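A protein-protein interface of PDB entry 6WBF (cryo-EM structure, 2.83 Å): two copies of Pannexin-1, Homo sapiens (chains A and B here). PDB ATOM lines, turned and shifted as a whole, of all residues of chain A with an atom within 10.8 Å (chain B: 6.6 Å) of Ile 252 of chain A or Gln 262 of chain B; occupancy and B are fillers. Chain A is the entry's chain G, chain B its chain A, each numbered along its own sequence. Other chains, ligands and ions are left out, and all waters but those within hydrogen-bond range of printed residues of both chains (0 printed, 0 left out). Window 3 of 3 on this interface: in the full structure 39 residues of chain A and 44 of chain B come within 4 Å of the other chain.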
ATOM      1  N   GLN A  76       8.544  20.193  35.269  1.00  0.00           N
ATOM      2  CA  GLN A  76       9.445  21.323  35.074  1.00  0.00           C
ATOM      3  C   GLN A  76      10.448  21.424  36.212  1.00  0.00           C
ATOM      4  O   GLN A  76      11.633  21.698  35.989  1.00  0.00           O
ATOM      5  CB  GLN A  76       8.644  22.613  34.951  1.00  0.00           C
ATOM      6  CG  GLN A  76       7.833  22.712  33.686  1.00  0.00           C
ATOM      7  CD  GLN A  76       7.246  24.083  33.501  1.00  0.00           C
ATOM      8  OE1 GLN A  76       7.506  24.755  32.508  1.00  0.00           O
ATOM      9  NE2 GLN A  76       6.454  24.517  34.466  1.00  0.00           N
ATOM     10  N   PHE A  79      12.964  18.822  35.688  1.00  0.00           N
ATOM     11  CA  PHE A  79      13.918  19.265  34.682  1.00  0.00           C
ATOM     12  C   PHE A  79      14.941  20.204  35.283  1.00  0.00           C
ATOM     13  O   PHE A  79      16.127  20.113  34.966  1.00  0.00           O
ATOM     14  CB  PHE A  79      13.216  19.963  33.521  1.00  0.00           C
ATOM     15  CG  PHE A  79      14.165  20.627  32.566  1.00  0.00           C
ATOM     16  CD1 PHE A  79      14.786  19.901  31.573  1.00  0.00           C
ATOM     17  CD2 PHE A  79      14.444  21.975  32.664  1.00  0.00           C
ATOM     18  CE1 PHE A  79      15.657  20.503  30.697  1.00  0.00           C
ATOM     19  CE2 PHE A  79      15.315  22.577  31.791  1.00  0.00           C
ATOM     20  CZ  PHE A  79      15.922  21.840  30.806  1.00  0.00           C
ATOM     21  N   TYR A  83      18.784  19.276  35.257  1.00  0.00           N
ATOM     22  CA  TYR A  83      19.626  20.179  34.488  1.00  0.00           C
ATOM     23  C   TYR A  83      20.752  20.718  35.343  1.00  0.00           C
ATOM     24  O   TYR A  83      21.901  20.755  34.911  1.00  0.00           O
ATOM     25  CB  TYR A  83      18.800  21.332  33.923  1.00  0.00           C
ATOM     26  CG  TYR A  83      19.550  22.209  32.939  1.00  0.00           C
ATOM     27  CD1 TYR A  83      20.579  23.041  33.355  1.00  0.00           C
ATOM     28  CD2 TYR A  83      19.212  22.219  31.601  1.00  0.00           C
ATOM     29  CE1 TYR A  83      21.254  23.837  32.468  1.00  0.00           C
ATOM     30  CE2 TYR A  83      19.884  23.014  30.704  1.00  0.00           C
ATOM     31  CZ  TYR A  83      20.903  23.822  31.145  1.00  0.00           C
ATOM     32  OH  TYR A  83      21.578  24.620  30.254  1.00  0.00           O
ATOM     33  N   SER A 247      21.190  28.282  36.418  1.00  0.00           N
ATOM     34  CA  SER A 247      20.350  29.000  35.474  1.00  0.00           C
ATOM     35  C   SER A 247      20.097  28.123  34.258  1.00  0.00           C
ATOM     36  O   SER A 247      21.026  27.835  33.494  1.00  0.00           O
ATOM     37  CB  SER A 247      21.014  30.311  35.060  1.00  0.00           C
ATOM     38  OG  SER A 247      20.226  31.005  34.114  1.00  0.00           O
ATOM     39  N   ILE A 248      18.849  27.697  34.076  1.00  0.00           N
ATOM     40  CA  ILE A 248      18.507  26.919  32.891  1.00  0.00           C
ATOM     41  C   ILE A 248      18.092  27.884  31.786  1.00  0.00           C
ATOM     42  O   ILE A 248      16.907  28.063  31.498  1.00  0.00           O
ATOM     43  CB  ILE A 248      17.414  25.878  33.203  1.00  0.00           C
ATOM     44  CG1 ILE A 248      16.162  26.521  33.788  1.00  0.00           C
ATOM     45  CG2 ILE A 248      17.909  24.903  34.228  1.00  0.00           C
ATOM     46  CD1 ILE A 248      14.903  25.785  33.426  1.00  0.00           C
ATOM     47  N   LYS A 249      19.075  28.502  31.138  1.00  0.00           N
ATOM     48  CA  LYS A 249      18.805  29.511  30.124  1.00  0.00           C
ATOM     49  C   LYS A 249      19.723  29.374  28.919  1.00  0.00           C
ATOM     50  O   LYS A 249      20.064  30.385  28.295  1.00  0.00           O
ATOM     51  CB  LYS A 249      18.920  30.918  30.717  1.00  0.00           C
ATOM     52  CG  LYS A 249      18.003  31.168  31.897  1.00  0.00           C
ATOM     53  CD  LYS A 249      16.566  31.398  31.473  1.00  0.00           C
ATOM     54  CE  LYS A 249      16.317  32.863  31.184  1.00  0.00           C
ATOM     55  NZ  LYS A 249      14.867  33.155  31.052  1.00  0.00           N
ATOM     56  N   SER A 250      20.159  28.165  28.599  1.00  0.00           N
ATOM     57  CA  SER A 250      20.847  27.931  27.345  1.00  0.00           C
ATOM     58  C   SER A 250      19.869  27.380  26.315  1.00  0.00           C
ATOM     59  O   SER A 250      18.835  26.805  26.656  1.00  0.00           O
ATOM     60  CB  SER A 250      22.006  26.961  27.546  1.00  0.00           C
ATOM     61  OG  SER A 250      21.530  25.707  27.994  1.00  0.00           O
ATOM     62  N   GLY A 251      20.202  27.562  25.043  1.00  0.00           N
ATOM     63  CA  GLY A 251      19.316  27.103  23.993  1.00  0.00           C
ATOM     64  C   GLY A 251      18.095  27.995  23.855  1.00  0.00           C
ATOM     65  O   GLY A 251      18.148  29.202  24.081  1.00  0.00           O
ATOM     66  N   ILE A 252      16.974  27.374  23.479  1.00  0.00           N
ATOM     67  CA  ILE A 252      15.751  28.131  23.251  1.00  0.00           C
ATOM     68  C   ILE A 252      15.189  28.712  24.539  1.00  0.00           C
ATOM     69  O   ILE A 252      14.320  29.588  24.490  1.00  0.00           O
ATOM     70  CB  ILE A 252      14.699  27.251  22.561  1.00  0.00           C
ATOM     71  CG1 ILE A 252      14.176  26.196  23.531  1.00  0.00           C
ATOM     72  CG2 ILE A 252      15.287  26.589  21.337  1.00  0.00           C
ATOM     73  CD1 ILE A 252      13.078  25.348  22.961  1.00  0.00           C
ATOM     74  N   LEU A 253      15.656  28.246  25.697  1.00  0.00           N
ATOM     75  CA  LEU A 253      15.166  28.793  26.957  1.00  0.00           C
ATOM     76  C   LEU A 253      15.830  30.125  27.278  1.00  0.00           C
ATOM     77  O   LEU A 253      15.460  30.790  28.249  1.00  0.00           O
ATOM     78  CB  LEU A 253      15.407  27.799  28.087  1.00  0.00           C
ATOM     79  CG  LEU A 253      14.518  26.565  28.080  1.00  0.00           C
ATOM     80  CD1 LEU A 253      14.853  25.679  29.261  1.00  0.00           C
ATOM     81  CD2 LEU A 253      13.070  26.982  28.117  1.00  0.00           C
ATOM     82  N   ARG A 254      16.816  30.525  26.472  1.00  0.00           N
ATOM     83  CA  ARG A 254      17.630  31.690  26.809  1.00  0.00           C
ATOM     84  C   ARG A 254      16.780  32.944  26.953  1.00  0.00           C
ATOM     85  O   ARG A 254      16.849  33.639  27.971  1.00  0.00           O
ATOM     86  CB  ARG A 254      18.715  31.893  25.756  1.00  0.00           C
ATOM     87  CG  ARG A 254      19.690  33.005  26.090  1.00  0.00           C
ATOM     88  CD  ARG A 254      20.861  33.013  25.126  1.00  0.00           C
ATOM     89  NE  ARG A 254      21.669  31.803  25.244  1.00  0.00           N
ATOM     90  CZ  ARG A 254      21.711  30.840  24.331  1.00  0.00           C
ATOM     91  NH1 ARG A 254      22.474  29.773  24.522  1.00  0.00           N
ATOM     92  NH2 ARG A 254      20.988  30.940  23.225  1.00  0.00           N
ATOM     93  N   ASN A 255      15.973  33.253  25.941  1.00  0.00           N
ATOM     94  CA  ASN A 255      15.179  34.473  26.005  1.00  0.00           C
ATOM     95  C   ASN A 255      13.759  34.192  26.476  1.00  0.00           C
ATOM     96  O   ASN A 255      12.895  35.076  26.414  1.00  0.00           O
ATOM     97  CB  ASN A 255      15.185  35.175  24.649  1.00  0.00           C
ATOM     98  CG  ASN A 255      14.707  34.282  23.515  1.00  0.00           C
ATOM     99  OD1 ASN A 255      13.758  33.514  23.666  1.00  0.00           O
ATOM    100  ND2 ASN A 255      15.372  34.381  22.365  1.00  0.00           N
ATOM    101  N   ASP A 256      13.491  32.970  26.931  1.00  0.00           N
ATOM    102  CA  ASP A 256      12.191  32.647  27.501  1.00  0.00           C
ATOM    103  C   ASP A 256      11.939  33.488  28.745  1.00  0.00           C
ATOM    104  O   ASP A 256      12.872  33.862  29.455  1.00  0.00           O
ATOM    105  CB  ASP A 256      12.118  31.158  27.840  1.00  0.00           C
ATOM    106  CG  ASP A 256      10.698  30.669  28.026  1.00  0.00           C
ATOM    107  OD1 ASP A 256       9.847  31.461  28.477  1.00  0.00           O
ATOM    108  OD2 ASP A 256      10.430  29.491  27.716  1.00  0.00           O
ATOM    109  N   SER A 257      10.666  33.783  29.004  1.00  0.00           N
ATOM    110  CA  SER A 257      10.307  34.686  30.090  1.00  0.00           C
ATOM    111  C   SER A 257       9.639  33.995  31.269  1.00  0.00           C
ATOM    112  O   SER A 257       9.786  34.468  32.400  1.00  0.00           O
ATOM    113  CB  SER A 257       9.381  35.790  29.570  1.00  0.00           C
ATOM    114  OG  SER A 257      10.043  36.598  28.614  1.00  0.00           O
ATOM    115  N   THR A 258       8.915  32.899  31.042  1.00  0.00           N
ATOM    116  CA  THR A 258       8.230  32.234  32.144  1.00  0.00           C
ATOM    117  C   THR A 258       9.220  31.589  33.103  1.00  0.00           C
ATOM    118  O   THR A 258       8.934  31.433  34.294  1.00  0.00           O
ATOM    119  CB  THR A 258       7.253  31.188  31.609  1.00  0.00           C
ATOM    120  OG1 THR A 258       6.681  30.465  32.705  1.00  0.00           O
ATOM    121  CG2 THR A 258       7.961  30.211  30.683  1.00  0.00           C
ATOM    122  N   VAL A 259      10.389  31.206  32.603  1.00  0.00           N
ATOM    123  CA  VAL A 259      11.420  30.576  33.421  1.00  0.00           C
ATOM    124  C   VAL A 259      12.221  31.659  34.135  1.00  0.00           C
ATOM    125  O   VAL A 259      12.659  32.628  33.500  1.00  0.00           O
ATOM    126  CB  VAL A 259      12.312  29.660  32.566  1.00  0.00           C
ATOM    127  CG1 VAL A 259      12.924  30.424  31.412  1.00  0.00           C
ATOM    128  CG2 VAL A 259      13.394  29.043  33.417  1.00  0.00           C
ATOM    129  N   PHE B  67      11.792  19.798  29.732  1.00  0.00           N
ATOM    130  CA  PHE B  67      11.169  21.069  30.087  1.00  0.00           C
ATOM    131  C   PHE B  67       9.979  21.417  29.205  1.00  0.00           C
ATOM    132  O   PHE B  67      10.048  22.346  28.395  1.00  0.00           O
ATOM    133  CB  PHE B  67      12.171  22.221  30.042  1.00  0.00           C
ATOM    134  CG  PHE B  67      11.665  23.465  30.702  1.00  0.00           C
ATOM    135  CD1 PHE B  67      11.556  23.533  32.075  1.00  0.00           C
ATOM    136  CD2 PHE B  67      11.269  24.551  29.954  1.00  0.00           C
ATOM    137  CE1 PHE B  67      11.079  24.659  32.684  1.00  0.00           C
ATOM    138  CE2 PHE B  67      10.786  25.678  30.565  1.00  0.00           C
ATOM    139  CZ  PHE B  67      10.692  25.729  31.930  1.00  0.00           C
ATOM    140  N   GLN B  95      16.898  19.395  16.337  1.00  0.00           N
ATOM    141  CA  GLN B  95      17.870  20.322  15.774  1.00  0.00           C
ATOM    142  C   GLN B  95      18.920  20.617  16.836  1.00  0.00           C
ATOM    143  O   GLN B  95      18.609  21.225  17.865  1.00  0.00           O
ATOM    144  CB  GLN B  95      17.194  21.610  15.307  1.00  0.00           C
ATOM    145  N   VAL B 245      17.498  20.684  20.787  1.00  0.00           N
ATOM    146  CA  VAL B 245      16.138  21.176  20.638  1.00  0.00           C
ATOM    147  C   VAL B 245      15.330  20.094  19.945  1.00  0.00           C
ATOM    148  O   VAL B 245      15.742  19.570  18.908  1.00  0.00           O
ATOM    149  CB  VAL B 245      16.110  22.487  19.845  1.00  0.00           C
ATOM    150  CG1 VAL B 245      14.727  23.071  19.863  1.00  0.00           C
ATOM    151  CG2 VAL B 245      17.108  23.464  20.421  1.00  0.00           C
ATOM    152  N   CYS B 246      14.181  19.758  20.515  1.00  0.00           N
ATOM    153  CA  CYS B 246      13.360  18.653  20.048  1.00  0.00           C
ATOM    154  C   CYS B 246      11.946  19.152  19.801  1.00  0.00           C
ATOM    155  O   CYS B 246      11.440  19.990  20.552  1.00  0.00           O
ATOM    156  CB  CYS B 246      13.360  17.518  21.067  1.00  0.00           C
ATOM    157  SG  CYS B 246      12.025  16.337  20.898  1.00  0.00           S
ATOM    158  N   SER B 247      11.318  18.643  18.750  1.00  0.00           N
ATOM    159  CA  SER B 247      10.011  19.110  18.319  1.00  0.00           C
ATOM    160  C   SER B 247       9.086  17.915  18.132  1.00  0.00           C
ATOM    161  O   SER B 247       9.298  17.101  17.228  1.00  0.00           O
ATOM    162  CB  SER B 247      10.130  19.901  17.019  1.00  0.00           C
ATOM    163  OG  SER B 247       8.862  20.333  16.567  1.00  0.00           O
ATOM    164  N   ILE B 248       8.067  17.809  18.981  1.00  0.00           N
ATOM    165  CA  ILE B 248       7.090  16.739  18.821  1.00  0.00           C
ATOM    166  C   ILE B 248       5.975  17.240  17.911  1.00  0.00           C
ATOM    167  O   ILE B 248       4.885  17.598  18.362  1.00  0.00           O
ATOM    168  CB  ILE B 248       6.561  16.256  20.186  1.00  0.00           C
ATOM    169  CG1 ILE B 248       5.963  17.394  21.004  1.00  0.00           C
ATOM    170  CG2 ILE B 248       7.683  15.690  21.002  1.00  0.00           C
ATOM    171  CD1 ILE B 248       4.841  16.945  21.897  1.00  0.00           C
ATOM    172  N   LYS B 249       6.233  17.247  16.606  1.00  0.00           N
ATOM    173  CA  LYS B 249       5.282  17.785  15.642  1.00  0.00           C
ATOM    174  C   LYS B 249       5.182  16.924  14.394  1.00  0.00           C
ATOM    175  O   LYS B 249       4.946  17.456  13.303  1.00  0.00           O
ATOM    176  CB  LYS B 249       5.650  19.221  15.264  1.00  0.00           C
ATOM    177  CG  LYS B 249       5.725  20.173  16.444  1.00  0.00           C
ATOM    178  CD  LYS B 249       4.355  20.588  16.939  1.00  0.00           C
ATOM    179  CE  LYS B 249       3.864  21.813  16.200  1.00  0.00           C
ATOM    180  NZ  LYS B 249       2.671  22.406  16.855  1.00  0.00           N
ATOM    181  N   VAL B 259       0.505  22.556  21.497  1.00  0.00           N
ATOM    182  CA  VAL B 259       1.865  22.062  21.689  1.00  0.00           C
ATOM    183  C   VAL B 259       2.850  23.081  21.126  1.00  0.00           C
ATOM    184  O   VAL B 259       2.681  23.547  19.993  1.00  0.00           O
ATOM    185  CB  VAL B 259       2.036  20.673  21.053  1.00  0.00           C
ATOM    186  CG1 VAL B 259       1.671  20.701  19.585  1.00  0.00           C
ATOM    187  CG2 VAL B 259       3.454  20.189  21.231  1.00  0.00           C
ATOM    188  N   PRO B 260       3.871  23.477  21.883  1.00  0.00           N
ATOM    189  CA  PRO B 260       4.828  24.460  21.372  1.00  0.00           C
ATOM    190  C   PRO B 260       5.670  23.889  20.244  1.00  0.00           C
ATOM    191  O   PRO B 260       5.738  22.678  20.028  1.00  0.00           O
ATOM    192  CB  PRO B 260       5.691  24.787  22.593  1.00  0.00           C
ATOM    193  CG  PRO B 260       5.553  23.613  23.470  1.00  0.00           C
ATOM    194  CD  PRO B 260       4.156  23.112  23.277  1.00  0.00           C
ATOM    195  N   ASP B 261       6.322  24.798  19.520  1.00  0.00           N
ATOM    196  CA  ASP B 261       7.045  24.403  18.317  1.00  0.00           C
ATOM    197  C   ASP B 261       8.218  23.494  18.640  1.00  0.00           C
ATOM    198  O   ASP B 261       8.491  22.538  17.906  1.00  0.00           O
ATOM    199  CB  ASP B 261       7.518  25.639  17.562  1.00  0.00           C
ATOM    200  CG  ASP B 261       6.377  26.399  16.927  1.00  0.00           C
ATOM    201  OD1 ASP B 261       5.368  25.761  16.572  1.00  0.00           O
ATOM    202  OD2 ASP B 261       6.490  27.634  16.780  1.00  0.00           O
ATOM    203  N   GLN B 262       8.926  23.768  19.731  1.00  0.00           N
ATOM    204  CA  GLN B 262      10.128  23.018  20.051  1.00  0.00           C
ATOM    205  C   GLN B 262      10.374  23.038  21.549  1.00  0.00           C
ATOM    206  O   GLN B 262       9.986  23.974  22.248  1.00  0.00           O
ATOM    207  CB  GLN B 262      11.338  23.583  19.314  1.00  0.00           C
ATOM    208  CG  GLN B 262      11.472  25.081  19.420  1.00  0.00           C
ATOM    209  CD  GLN B 262      12.499  25.627  18.456  1.00  0.00           C
ATOM    210  OE1 GLN B 262      12.871  24.964  17.490  1.00  0.00           O
ATOM    211  NE2 GLN B 262      12.969  26.838  18.716  1.00  0.00           N
ATOM    212  N   PHE B 263      11.035  21.991  22.030  1.00  0.00           N
ATOM    213  CA  PHE B 263      11.336  21.818  23.441  1.00  0.00           C
ATOM    214  C   PHE B 263      12.840  21.808  23.647  1.00  0.00           C
ATOM    215  O   PHE B 263      13.586  21.319  22.796  1.00  0.00           O
ATOM    216  CB  PHE B 263      10.743  20.519  23.972  1.00  0.00           C
ATOM    217  CG  PHE B 263       9.255  20.458  23.891  1.00  0.00           C
ATOM    218  CD1 PHE B 263       8.625  20.145  22.708  1.00  0.00           C
ATOM    219  CD2 PHE B 263       8.486  20.708  25.003  1.00  0.00           C
ATOM    220  CE1 PHE B 263       7.260  20.090  22.636  1.00  0.00           C
ATOM    221  CE2 PHE B 263       7.122  20.652  24.935  1.00  0.00           C
ATOM    222  CZ  PHE B 263       6.509  20.340  23.751  1.00  0.00           C
ATOM    223  N   GLN B 264      13.282  22.344  24.777  1.00  0.00           N
ATOM    224  CA  GLN B 264      14.703  22.349  25.119  1.00  0.00           C
ATOM    225  C   GLN B 264      14.982  21.125  25.976  1.00  0.00           C
ATOM    226  O   GLN B 264      14.724  21.109  27.178  1.00  0.00           O
ATOM    227  CB  GLN B 264      15.085  23.632  25.840  1.00  0.00           C
ATOM    228  CG  GLN B 264      16.506  23.636  26.351  1.00  0.00           C
ATOM    229  CD  GLN B 264      17.515  23.619  25.233  1.00  0.00           C
ATOM    230  OE1 GLN B 264      17.397  24.368  24.266  1.00  0.00           O
ATOM    231  NE2 GLN B 264      18.517  22.763  25.353  1.00  0.00           N
ATOM    232  N   CYS B 265      15.518  20.085  25.352  1.00  0.00           N
ATOM    233  CA  CYS B 265      15.875  18.870  26.064  1.00  0.00           C
ATOM    234  C   CYS B 265      17.359  18.861  26.382  1.00  0.00           C
ATOM    235  O   CYS B 265      18.161  19.467  25.670  1.00  0.00           O
ATOM    236  CB  CYS B 265      15.511  17.640  25.235  1.00  0.00           C
ATOM    237  SG  CYS B 265      13.779  17.570  24.799  1.00  0.00           S
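OE1 of Gln 264 of chain B lies within hydrogen-bond range of N of Ile 252 of chain A (3.1 Å).
The side-chain hydroxyl (OH) of Tyr 83 of chain A lies within hydrogen-bond range of the side-chain hydroxyl (OG) of Ser 250 of chain A, at 2.5 Å. O of Gly 251 of chain A sits close to NH2 of Arg 254 of chain A (3.4 Å). O of Cys 246 of chain B lies within hydrogen-bond range of N of Phe 263 of chain B, at 2.5 Å. The backbone NH (N) of Gln 95 of chain B lies within hydrogen-bond range of the backbone carbonyl oxygen (O) of Val 245 of chain B, at 2.8 Å.
Printed residues of chain B within 4 Å of Gln 76 of chain A: Phe 67 (3.4 Å). Printed residues of chain B within 4 Å of Ser 250 of chain A: Gln 264 (3.7 Å). Of the printed residues of chain B, Leu 253 of chain A touches Phe 67 and Gln 264. Ser 257 of chain A touches none of the printed residues of chain B. Of the printed residues of chain A, Phe 67 of chain B touches Gln 76 (3.4 Å), Phe 79 (3.3 Å) and Leu 253 (3.5 Å). Val 245 of chain B touches just one residue of chain A: Ile 252. No residue of chain A comes within 4 Å of Ser 247 of chain B. Gln 262 of chain B touches just one residue of chain A: Ile 252. Of chain A, only Ile 252 (3.6 Å) comes within 4 Å of Phe 263 of chain B. Of the printed residues of chain A, Gln 264 of chain B touches Phe 79, Ser 250, Gly 251, Ile 252 and Leu 253. The nearest residue of chain B that does not touch Ile 252 of chain A is Cys 246 of chain B (6.1 Å). The nearest printed residue of chain B that does not touch Gln 76 of chain A is Phe 263 of chain B (8.6 Å).
Among the printed residues, merely in contact across the chains: Phe 79 of chain A with Phe 67 of chain B (3.3 Å), Gly 251 of chain A with Gln 264 of chain B (3.4 Å), Gln 76 of chain A with Phe 67 of chain B (3.4 Å), Ile 252 of chain A with Gln 262 of chain B (3.5 Å), Leu 253 of chain A with Phe 67 of chain B (3.5 Å), Ile 252 of chain A with Phe 263 of chain B (3.6 Å), Phe 79 of chain A with Gln 264 of chain B (3.7 Å), Ser 250 of chain A with Gln 264 of chain B (3.7 Å), Ile 252 of chain A with Val 245 of chain B (3.7 Å) and Leu 253 of chain A with Gln 264 of chain B (3.7 Å).
Hydrophobic or aromatic side chains of chain B within 4 Å of the printed part of chain A: Phe 67 and Val 245. Of the 16 printed residues of chain A, 6 touch a printed residue of chain B. Along chain A the printed residues that touch a printed residue of chain B span positions 76 to 253. Among the printed residues, 11 pairs touch across the chains.
4 positions are printed for both chains. Of the 11 pairs that touch across the chains among the printed residues, none has its exchanged pair printed and touching as well.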
